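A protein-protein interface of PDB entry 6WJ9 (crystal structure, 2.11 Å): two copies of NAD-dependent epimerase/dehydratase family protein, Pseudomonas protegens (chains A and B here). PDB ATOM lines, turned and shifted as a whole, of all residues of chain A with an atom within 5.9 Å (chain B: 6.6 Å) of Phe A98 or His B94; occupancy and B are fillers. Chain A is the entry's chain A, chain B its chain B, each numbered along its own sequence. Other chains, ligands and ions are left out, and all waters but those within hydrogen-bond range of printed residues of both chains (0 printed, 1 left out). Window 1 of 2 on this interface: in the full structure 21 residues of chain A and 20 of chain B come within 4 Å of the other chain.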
ATOM      1  N   THR A  93      20.868 -31.672 -21.967  1.00  0.00           N
ATOM      2  CA  THR A  93      20.348 -30.721 -22.952  1.00  0.00           C
ATOM      3  C   THR A  93      21.109 -29.397 -22.929  1.00  0.00           C
ATOM      4  O   THR A  93      21.160 -28.699 -23.955  1.00  0.00           O
ATOM      5  CB  THR A  93      18.847 -30.465 -22.744  1.00  0.00           C
ATOM      6  OG1 THR A  93      18.606 -29.960 -21.416  1.00  0.00           O
ATOM      7  CG2 THR A  93      18.041 -31.755 -22.975  1.00  0.00           C
ATOM      8  N   HIS A  94      21.701 -29.029 -21.787  1.00  0.00           N
ATOM      9  CA  HIS A  94      22.491 -27.801 -21.745  1.00  0.00           C
ATOM     10  C   HIS A  94      23.663 -27.853 -22.725  1.00  0.00           C
ATOM     11  O   HIS A  94      24.050 -26.817 -23.273  1.00  0.00           O
ATOM     12  CB  HIS A  94      22.996 -27.522 -20.321  1.00  0.00           C
ATOM     13  CG  HIS A  94      23.850 -26.294 -20.216  1.00  0.00           C
ATOM     14  ND1 HIS A  94      23.331 -25.018 -20.253  1.00  0.00           N
ATOM     15  CD2 HIS A  94      25.194 -26.149 -20.096  1.00  0.00           C
ATOM     16  CE1 HIS A  94      24.314 -24.140 -20.156  1.00  0.00           C
ATOM     17  NE2 HIS A  94      25.454 -24.802 -20.056  1.00  0.00           N
ATOM     18  N   GLN A  95      24.237 -29.038 -22.962  1.00  0.00           N
ATOM     19  CA  GLN A  95      25.300 -29.157 -23.958  1.00  0.00           C
ATOM     20  C   GLN A  95      24.787 -28.796 -25.349  1.00  0.00           C
ATOM     21  O   GLN A  95      25.435 -28.048 -26.089  1.00  0.00           O
ATOM     22  CB  GLN A  95      25.875 -30.581 -23.968  1.00  0.00           C
ATOM     23  CG  GLN A  95      26.497 -31.020 -22.664  1.00  0.00           C
ATOM     24  CD  GLN A  95      27.658 -30.134 -22.260  1.00  0.00           C
ATOM     25  OE1 GLN A  95      27.585 -29.410 -21.259  1.00  0.00           O
ATOM     26  NE2 GLN A  95      28.738 -30.179 -23.043  1.00  0.00           N
ATOM     27  N   SER A  96      23.621 -29.323 -25.725  1.00  0.00           N
ATOM     28  CA  SER A  96      23.064 -29.050 -27.050  1.00  0.00           C
ATOM     29  C   SER A  96      22.460 -27.653 -27.153  1.00  0.00           C
ATOM     30  O   SER A  96      22.560 -27.007 -28.206  1.00  0.00           O
ATOM     31  CB  SER A  96      22.000 -30.096 -27.399  1.00  0.00           C
ATOM     32  OG  SER A  96      22.592 -31.361 -27.651  1.00  0.00           O
ATOM     33  N   ASN A  97      21.813 -27.176 -26.094  1.00  0.00           N
ATOM     34  CA  ASN A  97      21.048 -25.932 -26.179  1.00  0.00           C
ATOM     35  C   ASN A  97      21.866 -24.690 -25.840  1.00  0.00           C
ATOM     36  O   ASN A  97      21.453 -23.579 -26.199  1.00  0.00           O
ATOM     37  CB  ASN A  97      19.817 -25.994 -25.259  1.00  0.00           C
ATOM     38  CG  ASN A  97      18.855 -27.112 -25.652  1.00  0.00           C
ATOM     39  OD1 ASN A  97      18.863 -27.561 -26.789  1.00  0.00           O
ATOM     40  ND2 ASN A  97      18.037 -27.569 -24.708  1.00  0.00           N
ATOM     41  N   PHE A  98      23.006 -24.837 -25.166  1.00  0.00           N
ATOM     42  CA  PHE A  98      23.851 -23.673 -24.944  1.00  0.00           C
ATOM     43  C   PHE A  98      25.304 -23.893 -25.357  1.00  0.00           C
ATOM     44  O   PHE A  98      25.892 -23.028 -26.012  1.00  0.00           O
ATOM     45  CB  PHE A  98      23.854 -23.211 -23.482  1.00  0.00           C
ATOM     46  CG  PHE A  98      24.891 -22.155 -23.236  1.00  0.00           C
ATOM     47  CD1 PHE A  98      24.648 -20.844 -23.607  1.00  0.00           C
ATOM     48  CD2 PHE A  98      26.146 -22.489 -22.756  1.00  0.00           C
ATOM     49  CE1 PHE A  98      25.615 -19.869 -23.446  1.00  0.00           C
ATOM     50  CE2 PHE A  98      27.130 -21.518 -22.604  1.00  0.00           C
ATOM     51  CZ  PHE A  98      26.867 -20.208 -22.947  1.00  0.00           C
ATOM     52  N   ILE A  99      25.919 -25.000 -24.929  1.00  0.00           N
ATOM     53  CA  ILE A  99      27.353 -25.173 -25.172  1.00  0.00           C
ATOM     54  C   ILE A  99      27.645 -25.135 -26.667  1.00  0.00           C
ATOM     55  O   ILE A  99      28.657 -24.569 -27.106  1.00  0.00           O
ATOM     56  CB  ILE A  99      27.859 -26.477 -24.521  1.00  0.00           C
ATOM     57  CG1 ILE A  99      27.701 -26.407 -22.997  1.00  0.00           C
ATOM     58  CG2 ILE A  99      29.336 -26.742 -24.895  1.00  0.00           C
ATOM     59  CD1 ILE A  99      28.680 -25.417 -22.319  1.00  0.00           C
ATOM     60  N   ALA A 100      26.752 -25.715 -27.477  1.00  0.00           N
ATOM     61  CA  ALA A 100      26.957 -25.689 -28.921  1.00  0.00           C
ATOM     62  C   ALA A 100      27.034 -24.255 -29.439  1.00  0.00           C
ATOM     63  O   ALA A 100      27.859 -23.947 -30.307  1.00  0.00           O
ATOM     64  CB  ALA A 100      25.848 -26.476 -29.628  1.00  0.00           C
ATOM     65  N   THR A 101      26.205 -23.356 -28.899  1.00  0.00           N
ATOM     66  CA  THR A 101      26.298 -21.943 -29.272  1.00  0.00           C
ATOM     67  C   THR A 101      27.653 -21.351 -28.879  1.00  0.00           C
ATOM     68  O   THR A 101      28.305 -20.671 -29.682  1.00  0.00           O
ATOM     69  CB  THR A 101      25.174 -21.141 -28.617  1.00  0.00           C
ATOM     70  OG1 THR A 101      23.908 -21.751 -28.890  1.00  0.00           O
ATOM     71  CG2 THR A 101      25.175 -19.693 -29.143  1.00  0.00           C
ATOM     72  N   LEU A 102      28.088 -21.584 -27.640  1.00  0.00           N
ATOM     73  CA  LEU A 102      29.394 -21.088 -27.208  1.00  0.00           C
ATOM     74  C   LEU A 102      30.516 -21.638 -28.084  1.00  0.00           C
ATOM     75  O   LEU A 102      31.394 -20.890 -28.540  1.00  0.00           O
ATOM     76  CB  LEU A 102      29.628 -21.456 -25.740  1.00  0.00           C
ATOM     77  CG  LEU A 102      31.016 -21.164 -25.151  1.00  0.00           C
ATOM     78  CD1 LEU A 102      31.376 -19.695 -25.255  1.00  0.00           C
ATOM     79  CD2 LEU A 102      31.079 -21.615 -23.688  1.00  0.00           C
ATOM     80  N   ARG A 103      30.508 -22.952 -28.325  1.00  0.00           N
ATOM     81  CA  ARG A 103      31.551 -23.549 -29.155  1.00  0.00           C
ATOM     82  C   ARG A 103      31.530 -22.962 -30.558  1.00  0.00           C
ATOM     83  O   ARG A 103      32.584 -22.781 -31.181  1.00  0.00           O
ATOM     84  CB  ARG A 103      31.377 -25.067 -29.213  1.00  0.00           C
ATOM     85  CG  ARG A 103      31.623 -25.787 -27.903  1.00  0.00           C
ATOM     86  CD  ARG A 103      33.092 -25.860 -27.572  1.00  0.00           C
ATOM     87  NE  ARG A 103      33.328 -26.617 -26.343  1.00  0.00           N
ATOM     88  CZ  ARG A 103      34.493 -26.662 -25.704  1.00  0.00           C
ATOM     89  NH1 ARG A 103      35.540 -25.994 -26.175  1.00  0.00           N
ATOM     90  NH2 ARG A 103      34.613 -27.375 -24.590  1.00  0.00           N
ATOM     91  N   ASP A 149      18.671 -21.604 -21.763  1.00  0.00           N
ATOM     92  CA  ASP A 149      19.813 -21.773 -22.656  1.00  0.00           C
ATOM     93  C   ASP A 149      19.657 -20.967 -23.941  1.00  0.00           C
ATOM     94  O   ASP A 149      20.653 -20.477 -24.483  1.00  0.00           O
ATOM     95  CB  ASP A 149      20.010 -23.250 -23.001  1.00  0.00           C
ATOM     96  CG  ASP A 149      20.490 -24.070 -21.814  1.00  0.00           C
ATOM     97  OD1 ASP A 149      20.869 -23.492 -20.767  1.00  0.00           O
ATOM     98  OD2 ASP A 149      20.477 -25.305 -21.934  1.00  0.00           O
ATOM     99  N   ALA A 152      20.500 -17.445 -22.805  1.00  0.00           N
ATOM    100  CA  ALA A 152      21.937 -17.362 -22.557  1.00  0.00           C
ATOM    101  C   ALA A 152      22.718 -17.347 -23.864  1.00  0.00           C
ATOM    102  O   ALA A 152      23.698 -16.601 -24.009  1.00  0.00           O
ATOM    103  CB  ALA A 152      22.391 -18.531 -21.683  1.00  0.00           C
ATOM    104  N   SER A 153      22.309 -18.185 -24.820  1.00  0.00           N
ATOM    105  CA  SER A 153      22.897 -18.143 -26.155  1.00  0.00           C
ATOM    106  C   SER A 153      22.822 -16.740 -26.744  1.00  0.00           C
ATOM    107  O   SER A 153      23.803 -16.255 -27.319  1.00  0.00           O
ATOM    108  CB  SER A 153      22.188 -19.143 -27.081  1.00  0.00           C
ATOM    109  OG  SER A 153      22.479 -20.495 -26.748  1.00  0.00           O
ATOM    110  N   TYR A 156      25.452 -14.526 -25.019  1.00  0.00           N
ATOM    111  CA  TYR A 156      26.815 -14.811 -25.455  1.00  0.00           C
ATOM    112  C   TYR A 156      27.044 -14.333 -26.882  1.00  0.00           C
ATOM    113  O   TYR A 156      28.101 -13.766 -27.187  1.00  0.00           O
ATOM    114  CB  TYR A 156      27.112 -16.304 -25.330  1.00  0.00           C
ATOM    115  CG  TYR A 156      27.687 -16.697 -23.994  1.00  0.00           C
ATOM    116  CD1 TYR A 156      26.890 -16.723 -22.854  1.00  0.00           C
ATOM    117  CD2 TYR A 156      29.032 -17.040 -23.870  1.00  0.00           C
ATOM    118  CE1 TYR A 156      27.418 -17.096 -21.625  1.00  0.00           C
ATOM    119  CE2 TYR A 156      29.575 -17.418 -22.648  1.00  0.00           C
ATOM    120  CZ  TYR A 156      28.762 -17.440 -21.531  1.00  0.00           C
ATOM    121  OH  TYR A 156      29.292 -17.815 -20.327  1.00  0.00           O
ATOM    122  N   SER B  86      36.545 -13.876 -17.386  1.00  0.00           N
ATOM    123  CA  SER B  86      35.538 -14.518 -18.222  1.00  0.00           C
ATOM    124  C   SER B  86      35.554 -13.964 -19.639  1.00  0.00           C
ATOM    125  O   SER B  86      35.155 -14.660 -20.579  1.00  0.00           O
ATOM    126  CB  SER B  86      34.151 -14.357 -17.604  1.00  0.00           C
ATOM    127  OG  SER B  86      33.607 -13.093 -17.923  1.00  0.00           O
ATOM    128  N   ASP B  89      38.473 -15.941 -21.220  1.00  0.00           N
ATOM    129  CA  ASP B  89      38.254 -17.382 -21.365  1.00  0.00           C
ATOM    130  C   ASP B  89      36.810 -17.741 -21.038  1.00  0.00           C
ATOM    131  O   ASP B  89      36.513 -18.309 -19.977  1.00  0.00           O
ATOM    132  CB  ASP B  89      39.237 -18.170 -20.494  1.00  0.00           C
ATOM    133  CG  ASP B  89      39.398 -19.613 -20.950  1.00  0.00           C
ATOM    134  OD1 ASP B  89      38.593 -20.078 -21.790  1.00  0.00           O
ATOM    135  OD2 ASP B  89      40.330 -20.288 -20.465  1.00  0.00           O
ATOM    136  N   PRO B  90      35.877 -17.439 -21.946  1.00  0.00           N
ATOM    137  CA  PRO B  90      34.467 -17.806 -21.711  1.00  0.00           C
ATOM    138  C   PRO B  90      34.241 -19.292 -21.488  1.00  0.00           C
ATOM    139  O   PRO B  90      33.429 -19.667 -20.633  1.00  0.00           O
ATOM    140  CB  PRO B  90      33.767 -17.321 -22.985  1.00  0.00           C
ATOM    141  CG  PRO B  90      34.657 -16.254 -23.527  1.00  0.00           C
ATOM    142  CD  PRO B  90      36.055 -16.648 -23.179  1.00  0.00           C
ATOM    143  N   VAL B  91      34.940 -20.154 -22.230  1.00  0.00           N
ATOM    144  CA  VAL B  91      34.692 -21.591 -22.133  1.00  0.00           C
ATOM    145  C   VAL B  91      35.075 -22.114 -20.754  1.00  0.00           C
ATOM    146  O   VAL B  91      34.292 -22.812 -20.101  1.00  0.00           O
ATOM    147  CB  VAL B  91      35.441 -22.337 -23.255  1.00  0.00           C
ATOM    148  CG1 VAL B  91      35.421 -23.841 -23.007  1.00  0.00           C
ATOM    149  CG2 VAL B  91      34.828 -22.010 -24.610  1.00  0.00           C
ATOM    150  N   ALA B  92      36.282 -21.781 -20.282  1.00  0.00           N
ATOM    151  CA  ALA B  92      36.726 -22.284 -18.985  1.00  0.00           C
ATOM    152  C   ALA B  92      35.908 -21.688 -17.843  1.00  0.00           C
ATOM    153  O   ALA B  92      35.483 -22.406 -16.931  1.00  0.00           O
ATOM    154  CB  ALA B  92      38.221 -22.003 -18.787  1.00  0.00           C
ATOM    155  N   THR B  93      35.674 -20.371 -17.868  1.00  0.00           N
ATOM    156  CA  THR B  93      34.958 -19.767 -16.750  1.00  0.00           C
ATOM    157  C   THR B  93      33.489 -20.172 -16.715  1.00  0.00           C
ATOM    158  O   THR B  93      32.880 -20.151 -15.639  1.00  0.00           O
ATOM    159  CB  THR B  93      35.084 -18.241 -16.771  1.00  0.00           C
ATOM    160  OG1 THR B  93      34.609 -17.727 -18.015  1.00  0.00           O
ATOM    161  CG2 THR B  93      36.551 -17.821 -16.559  1.00  0.00           C
ATOM    162  N   HIS B  94      32.896 -20.540 -17.860  1.00  0.00           N
ATOM    163  CA  HIS B  94      31.511 -21.010 -17.835  1.00  0.00           C
ATOM    164  C   HIS B  94      31.365 -22.268 -16.982  1.00  0.00           C
ATOM    165  O   HIS B  94      30.324 -22.473 -16.351  1.00  0.00           O
ATOM    166  CB  HIS B  94      31.007 -21.259 -19.258  1.00  0.00           C
ATOM    167  CG  HIS B  94      29.597 -21.764 -19.323  1.00  0.00           C
ATOM    168  ND1 HIS B  94      28.501 -20.947 -19.142  1.00  0.00           N
ATOM    169  CD2 HIS B  94      29.106 -23.005 -19.561  1.00  0.00           C
ATOM    170  CE1 HIS B  94      27.396 -21.661 -19.262  1.00  0.00           C
ATOM    171  NE2 HIS B  94      27.736 -22.916 -19.506  1.00  0.00           N
ATOM    172  N   GLN B  95      32.388 -23.118 -16.948  1.00  0.00           N
ATOM    173  CA  GLN B  95      32.363 -24.275 -16.060  1.00  0.00           C
ATOM    174  C   GLN B  95      32.237 -23.839 -14.605  1.00  0.00           C
ATOM    175  O   GLN B  95      31.424 -24.380 -13.845  1.00  0.00           O
ATOM    176  CB  GLN B  95      33.629 -25.122 -16.261  1.00  0.00           C
ATOM    177  CG  GLN B  95      33.747 -25.756 -17.646  1.00  0.00           C
ATOM    178  CD  GLN B  95      32.564 -26.671 -17.972  1.00  0.00           C
ATOM    179  OE1 GLN B  95      32.264 -27.605 -17.225  1.00  0.00           O
ATOM    180  NE2 GLN B  95      31.887 -26.398 -19.086  1.00  0.00           N
ATOM    181  N   SER B  96      33.038 -22.847 -14.203  1.00  0.00           N
ATOM    182  CA  SER B  96      33.018 -22.390 -12.819  1.00  0.00           C
ATOM    183  C   SER B  96      31.812 -21.502 -12.521  1.00  0.00           C
ATOM    184  O   SER B  96      31.257 -21.562 -11.416  1.00  0.00           O
ATOM    185  CB  SER B  96      34.322 -21.657 -12.498  1.00  0.00           C
ATOM    186  OG  SER B  96      35.414 -22.571 -12.470  1.00  0.00           O
ATOM    187  N   ASN B  97      31.390 -20.680 -13.486  1.00  0.00           N
ATOM    188  CA  ASN B  97      30.394 -19.653 -13.211  1.00  0.00           C
ATOM    189  C   ASN B  97      28.964 -20.109 -13.475  1.00  0.00           C
ATOM    190  O   ASN B  97      28.030 -19.469 -12.980  1.00  0.00           O
ATOM    191  CB  ASN B  97      30.688 -18.396 -14.038  1.00  0.00           C
ATOM    192  CG  ASN B  97      32.010 -17.763 -13.669  1.00  0.00           C
ATOM    193  OD1 ASN B  97      32.556 -18.048 -12.607  1.00  0.00           O
ATOM    194  ND2 ASN B  97      32.538 -16.912 -14.547  1.00  0.00           N
ATOM    195  N   PHE B  98      28.767 -21.190 -14.237  1.00  0.00           N
ATOM    196  CA  PHE B  98      27.419 -21.718 -14.404  1.00  0.00           C
ATOM    197  C   PHE B  98      27.317 -23.218 -14.163  1.00  0.00           C
ATOM    198  O   PHE B  98      26.367 -23.673 -13.518  1.00  0.00           O
ATOM    199  CB  PHE B  98      26.851 -21.442 -15.798  1.00  0.00           C
ATOM    200  CG  PHE B  98      25.567 -22.161 -16.026  1.00  0.00           C
ATOM    201  CD1 PHE B  98      24.390 -21.664 -15.488  1.00  0.00           C
ATOM    202  CD2 PHE B  98      25.543 -23.390 -16.684  1.00  0.00           C
ATOM    203  CE1 PHE B  98      23.197 -22.350 -15.642  1.00  0.00           C
ATOM    204  CE2 PHE B  98      24.363 -24.093 -16.830  1.00  0.00           C
ATOM    205  CZ  PHE B  98      23.181 -23.571 -16.319  1.00  0.00           C
ATOM    206  N   ILE B  99      28.235 -24.002 -14.736  1.00  0.00           N
ATOM    207  CA  ILE B  99      28.115 -25.453 -14.625  1.00  0.00           C
ATOM    208  C   ILE B  99      28.123 -25.871 -13.156  1.00  0.00           C
ATOM    209  O   ILE B  99      27.345 -26.739 -12.738  1.00  0.00           O
ATOM    210  CB  ILE B  99      29.223 -26.145 -15.440  1.00  0.00           C
ATOM    211  CG1 ILE B  99      29.083 -25.802 -16.931  1.00  0.00           C
ATOM    212  CG2 ILE B  99      29.187 -27.669 -15.243  1.00  0.00           C
ATOM    213  CD1 ILE B  99      27.826 -26.399 -17.595  1.00  0.00           C
ATOM    214  N   ALA B 100      28.956 -25.213 -12.339  1.00  0.00           N
ATOM    215  CA  ALA B 100      28.997 -25.518 -10.909  1.00  0.00           C
ATOM    216  C   ALA B 100      27.626 -25.348 -10.253  1.00  0.00           C
ATOM    217  O   ALA B 100      27.225 -26.166  -9.413  1.00  0.00           O
ATOM    218  CB  ALA B 100      30.030 -24.632 -10.219  1.00  0.00           C
ATOM    219  N   PRO B 145      30.518 -12.975 -20.213  1.00  0.00           N
ATOM    220  CA  PRO B 145      30.168 -14.355 -19.820  1.00  0.00           C
ATOM    221  C   PRO B 145      29.929 -14.521 -18.326  1.00  0.00           C
ATOM    222  O   PRO B 145      29.007 -15.250 -17.943  1.00  0.00           O
ATOM    223  CB  PRO B 145      31.376 -15.173 -20.304  1.00  0.00           C
ATOM    224  CG  PRO B 145      31.913 -14.386 -21.461  1.00  0.00           C
ATOM    225  CD  PRO B 145      31.707 -12.937 -21.087  1.00  0.00           C
ATOM    226  N   ASP B 149      26.412 -15.810 -16.928  1.00  0.00           N
ATOM    227  CA  ASP B 149      26.428 -17.068 -16.192  1.00  0.00           C
ATOM    228  C   ASP B 149      25.792 -16.920 -14.820  1.00  0.00           C
ATOM    229  O   ASP B 149      25.153 -17.859 -14.327  1.00  0.00           O
ATOM    230  CB  ASP B 149      27.863 -17.578 -16.046  1.00  0.00           C
ATOM    231  CG  ASP B 149      28.403 -18.192 -17.321  1.00  0.00           C
ATOM    232  OD1 ASP B 149      27.632 -18.364 -18.292  1.00  0.00           O
ATOM    233  OD2 ASP B 149      29.609 -18.506 -17.343  1.00  0.00           O
ATOM    234  N   ALA B 152      22.031 -16.823 -15.692  1.00  0.00           N
ATOM    235  CA  ALA B 152      21.601 -18.179 -16.026  1.00  0.00           C
ATOM    236  C   ALA B 152      21.512 -19.040 -14.773  1.00  0.00           C
ATOM    237  O   ALA B 152      20.583 -19.845 -14.622  1.00  0.00           O
ATOM    238  CB  ALA B 152      22.558 -18.803 -17.046  1.00  0.00           C
ATOM    239  N   TYR B 156      18.233 -21.191 -13.588  1.00  0.00           N
ATOM    240  CA  TYR B 156      18.227 -22.615 -13.273  1.00  0.00           C
ATOM    241  C   TYR B 156      17.834 -22.858 -11.826  1.00  0.00           C
ATOM    242  O   TYR B 156      17.127 -23.828 -11.526  1.00  0.00           O
ATOM    243  CB  TYR B 156      19.593 -23.229 -13.560  1.00  0.00           C
ATOM    244  CG  TYR B 156      19.727 -23.755 -14.972  1.00  0.00           C
ATOM    245  CD1 TYR B 156      19.797 -22.881 -16.056  1.00  0.00           C
ATOM    246  CD2 TYR B 156      19.792 -25.121 -15.219  1.00  0.00           C
ATOM    247  CE1 TYR B 156      19.929 -23.357 -17.353  1.00  0.00           C
ATOM    248  CE2 TYR B 156      19.920 -25.613 -16.516  1.00  0.00           C
ATOM    249  CZ  TYR B 156      19.985 -24.724 -17.576  1.00  0.00           C
ATOM    250  OH  TYR B 156      20.124 -25.198 -18.857  1.00  0.00           O
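His A94 touches Phe B98. CD2 of His A94 touches CD1 of Ile B99 (3.6 Å). OH of Tyr B156 touches ND1 of His A94, at 3.5 Å. CE2 of Phe A98 touches CE1 of His B94 (3.4 Å). CD1 of Ile A99 touches CD2 of His B94 (3.7 Å). Leu A102 touches Val B91 (CD2 to CG2, 3.9 Å). Val B91 touches Arg A103. Pro B145 touches Tyr A156.
Phe A98 touches just one residue of chain B: His B94 (3.4 Å). Of the printed residues of chain A, His B94 touches His A94, Phe A98, Ile A99 and Tyr A156. Printed residues of chain B within 4 Å of His A94: His B94 (3.0 Å), Phe B98 (3.3 Å), Ile B99 (3.6 Å) and Tyr B156 (3.5 Å). Printed residues of chain A within 4 Å of Val B91: Leu A102 (3.9 Å) and Arg A103 (3.8 Å). Printed residues of chain A within 4 Å of Tyr B156: His A94 (3.5 Å) and Asp A149 (2.7 Å). Printed residues of chain B within 4 Å of Tyr A156: His B94, Pro B145 and Asp B149. Of the printed residues of chain A, Asp B149 touches Tyr A156. Ala A152 touches none of the printed residues of chain B. Ala B100 touches none of the printed residues of chain A. The nearest residue of chain B that does not touch Phe A98 is Asp B149 (5.1 Å). The nearest printed residue of chain B that does not touch Ile A99 is Gln B95 (4.7 Å).
Hydrophobic or aromatic side chains of chain B within 4 Å of the printed part of chain A: Val B91, His B94, Phe B98, Ile B99, Pro B145 and Tyr B156. Among the printed residues, 12 pairs touch across the chains.
The backbone carbonyl oxygen of His A94 sits at hydrogen-bond distance from the backbone NH of Ile A99 (3.1 Å). A ring nitrogen (ND1) of His A94 lies within hydrogen-bond range of the side-chain carboxylate (OD1) of Asp A149 (2.9 Å). The backbone carbonyl oxygen of Asp A149 is in hydrogen-bond range of the side-chain hydroxyl of Ser A153 (2.9 Å). O of His B94 lies within hydrogen-bond range of N of Ile B99. The side-chain carboxylate (OD1) of Asp B149 is in hydrogen-bond range of a ring nitrogen (ND1) of His B94, at 2.9 Å.
His B94 touches its own counterpart, His A94. His A94 touches Phe B98, and with the chains exchanged Phe A98 touches His B94. His A94 touches Tyr B156, and with the chains exchanged Tyr A156 touches His B94. Asp A149 touches Tyr B156, and with the chains exchanged Tyr A156 touches Asp B149. 11 positions are printed for both chains.
NE2 of His A94 sits at hydrogen-bond distance from NE2 of His B94 (3.0 Å). The side-chain carboxylate of Asp A149 sits at hydrogen-bond distance from the side-chain hydroxyl of Tyr B156, 2.7 Å away. A ring nitrogen (ND1) of His B94 sits at hydrogen-bond distance from the side-chain hydroxyl (OH) of Tyr A156, at 3.4 Å. OH of Tyr A156 lies within hydrogen-bond range of OD1 of Asp B149, 2.7 Å away.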
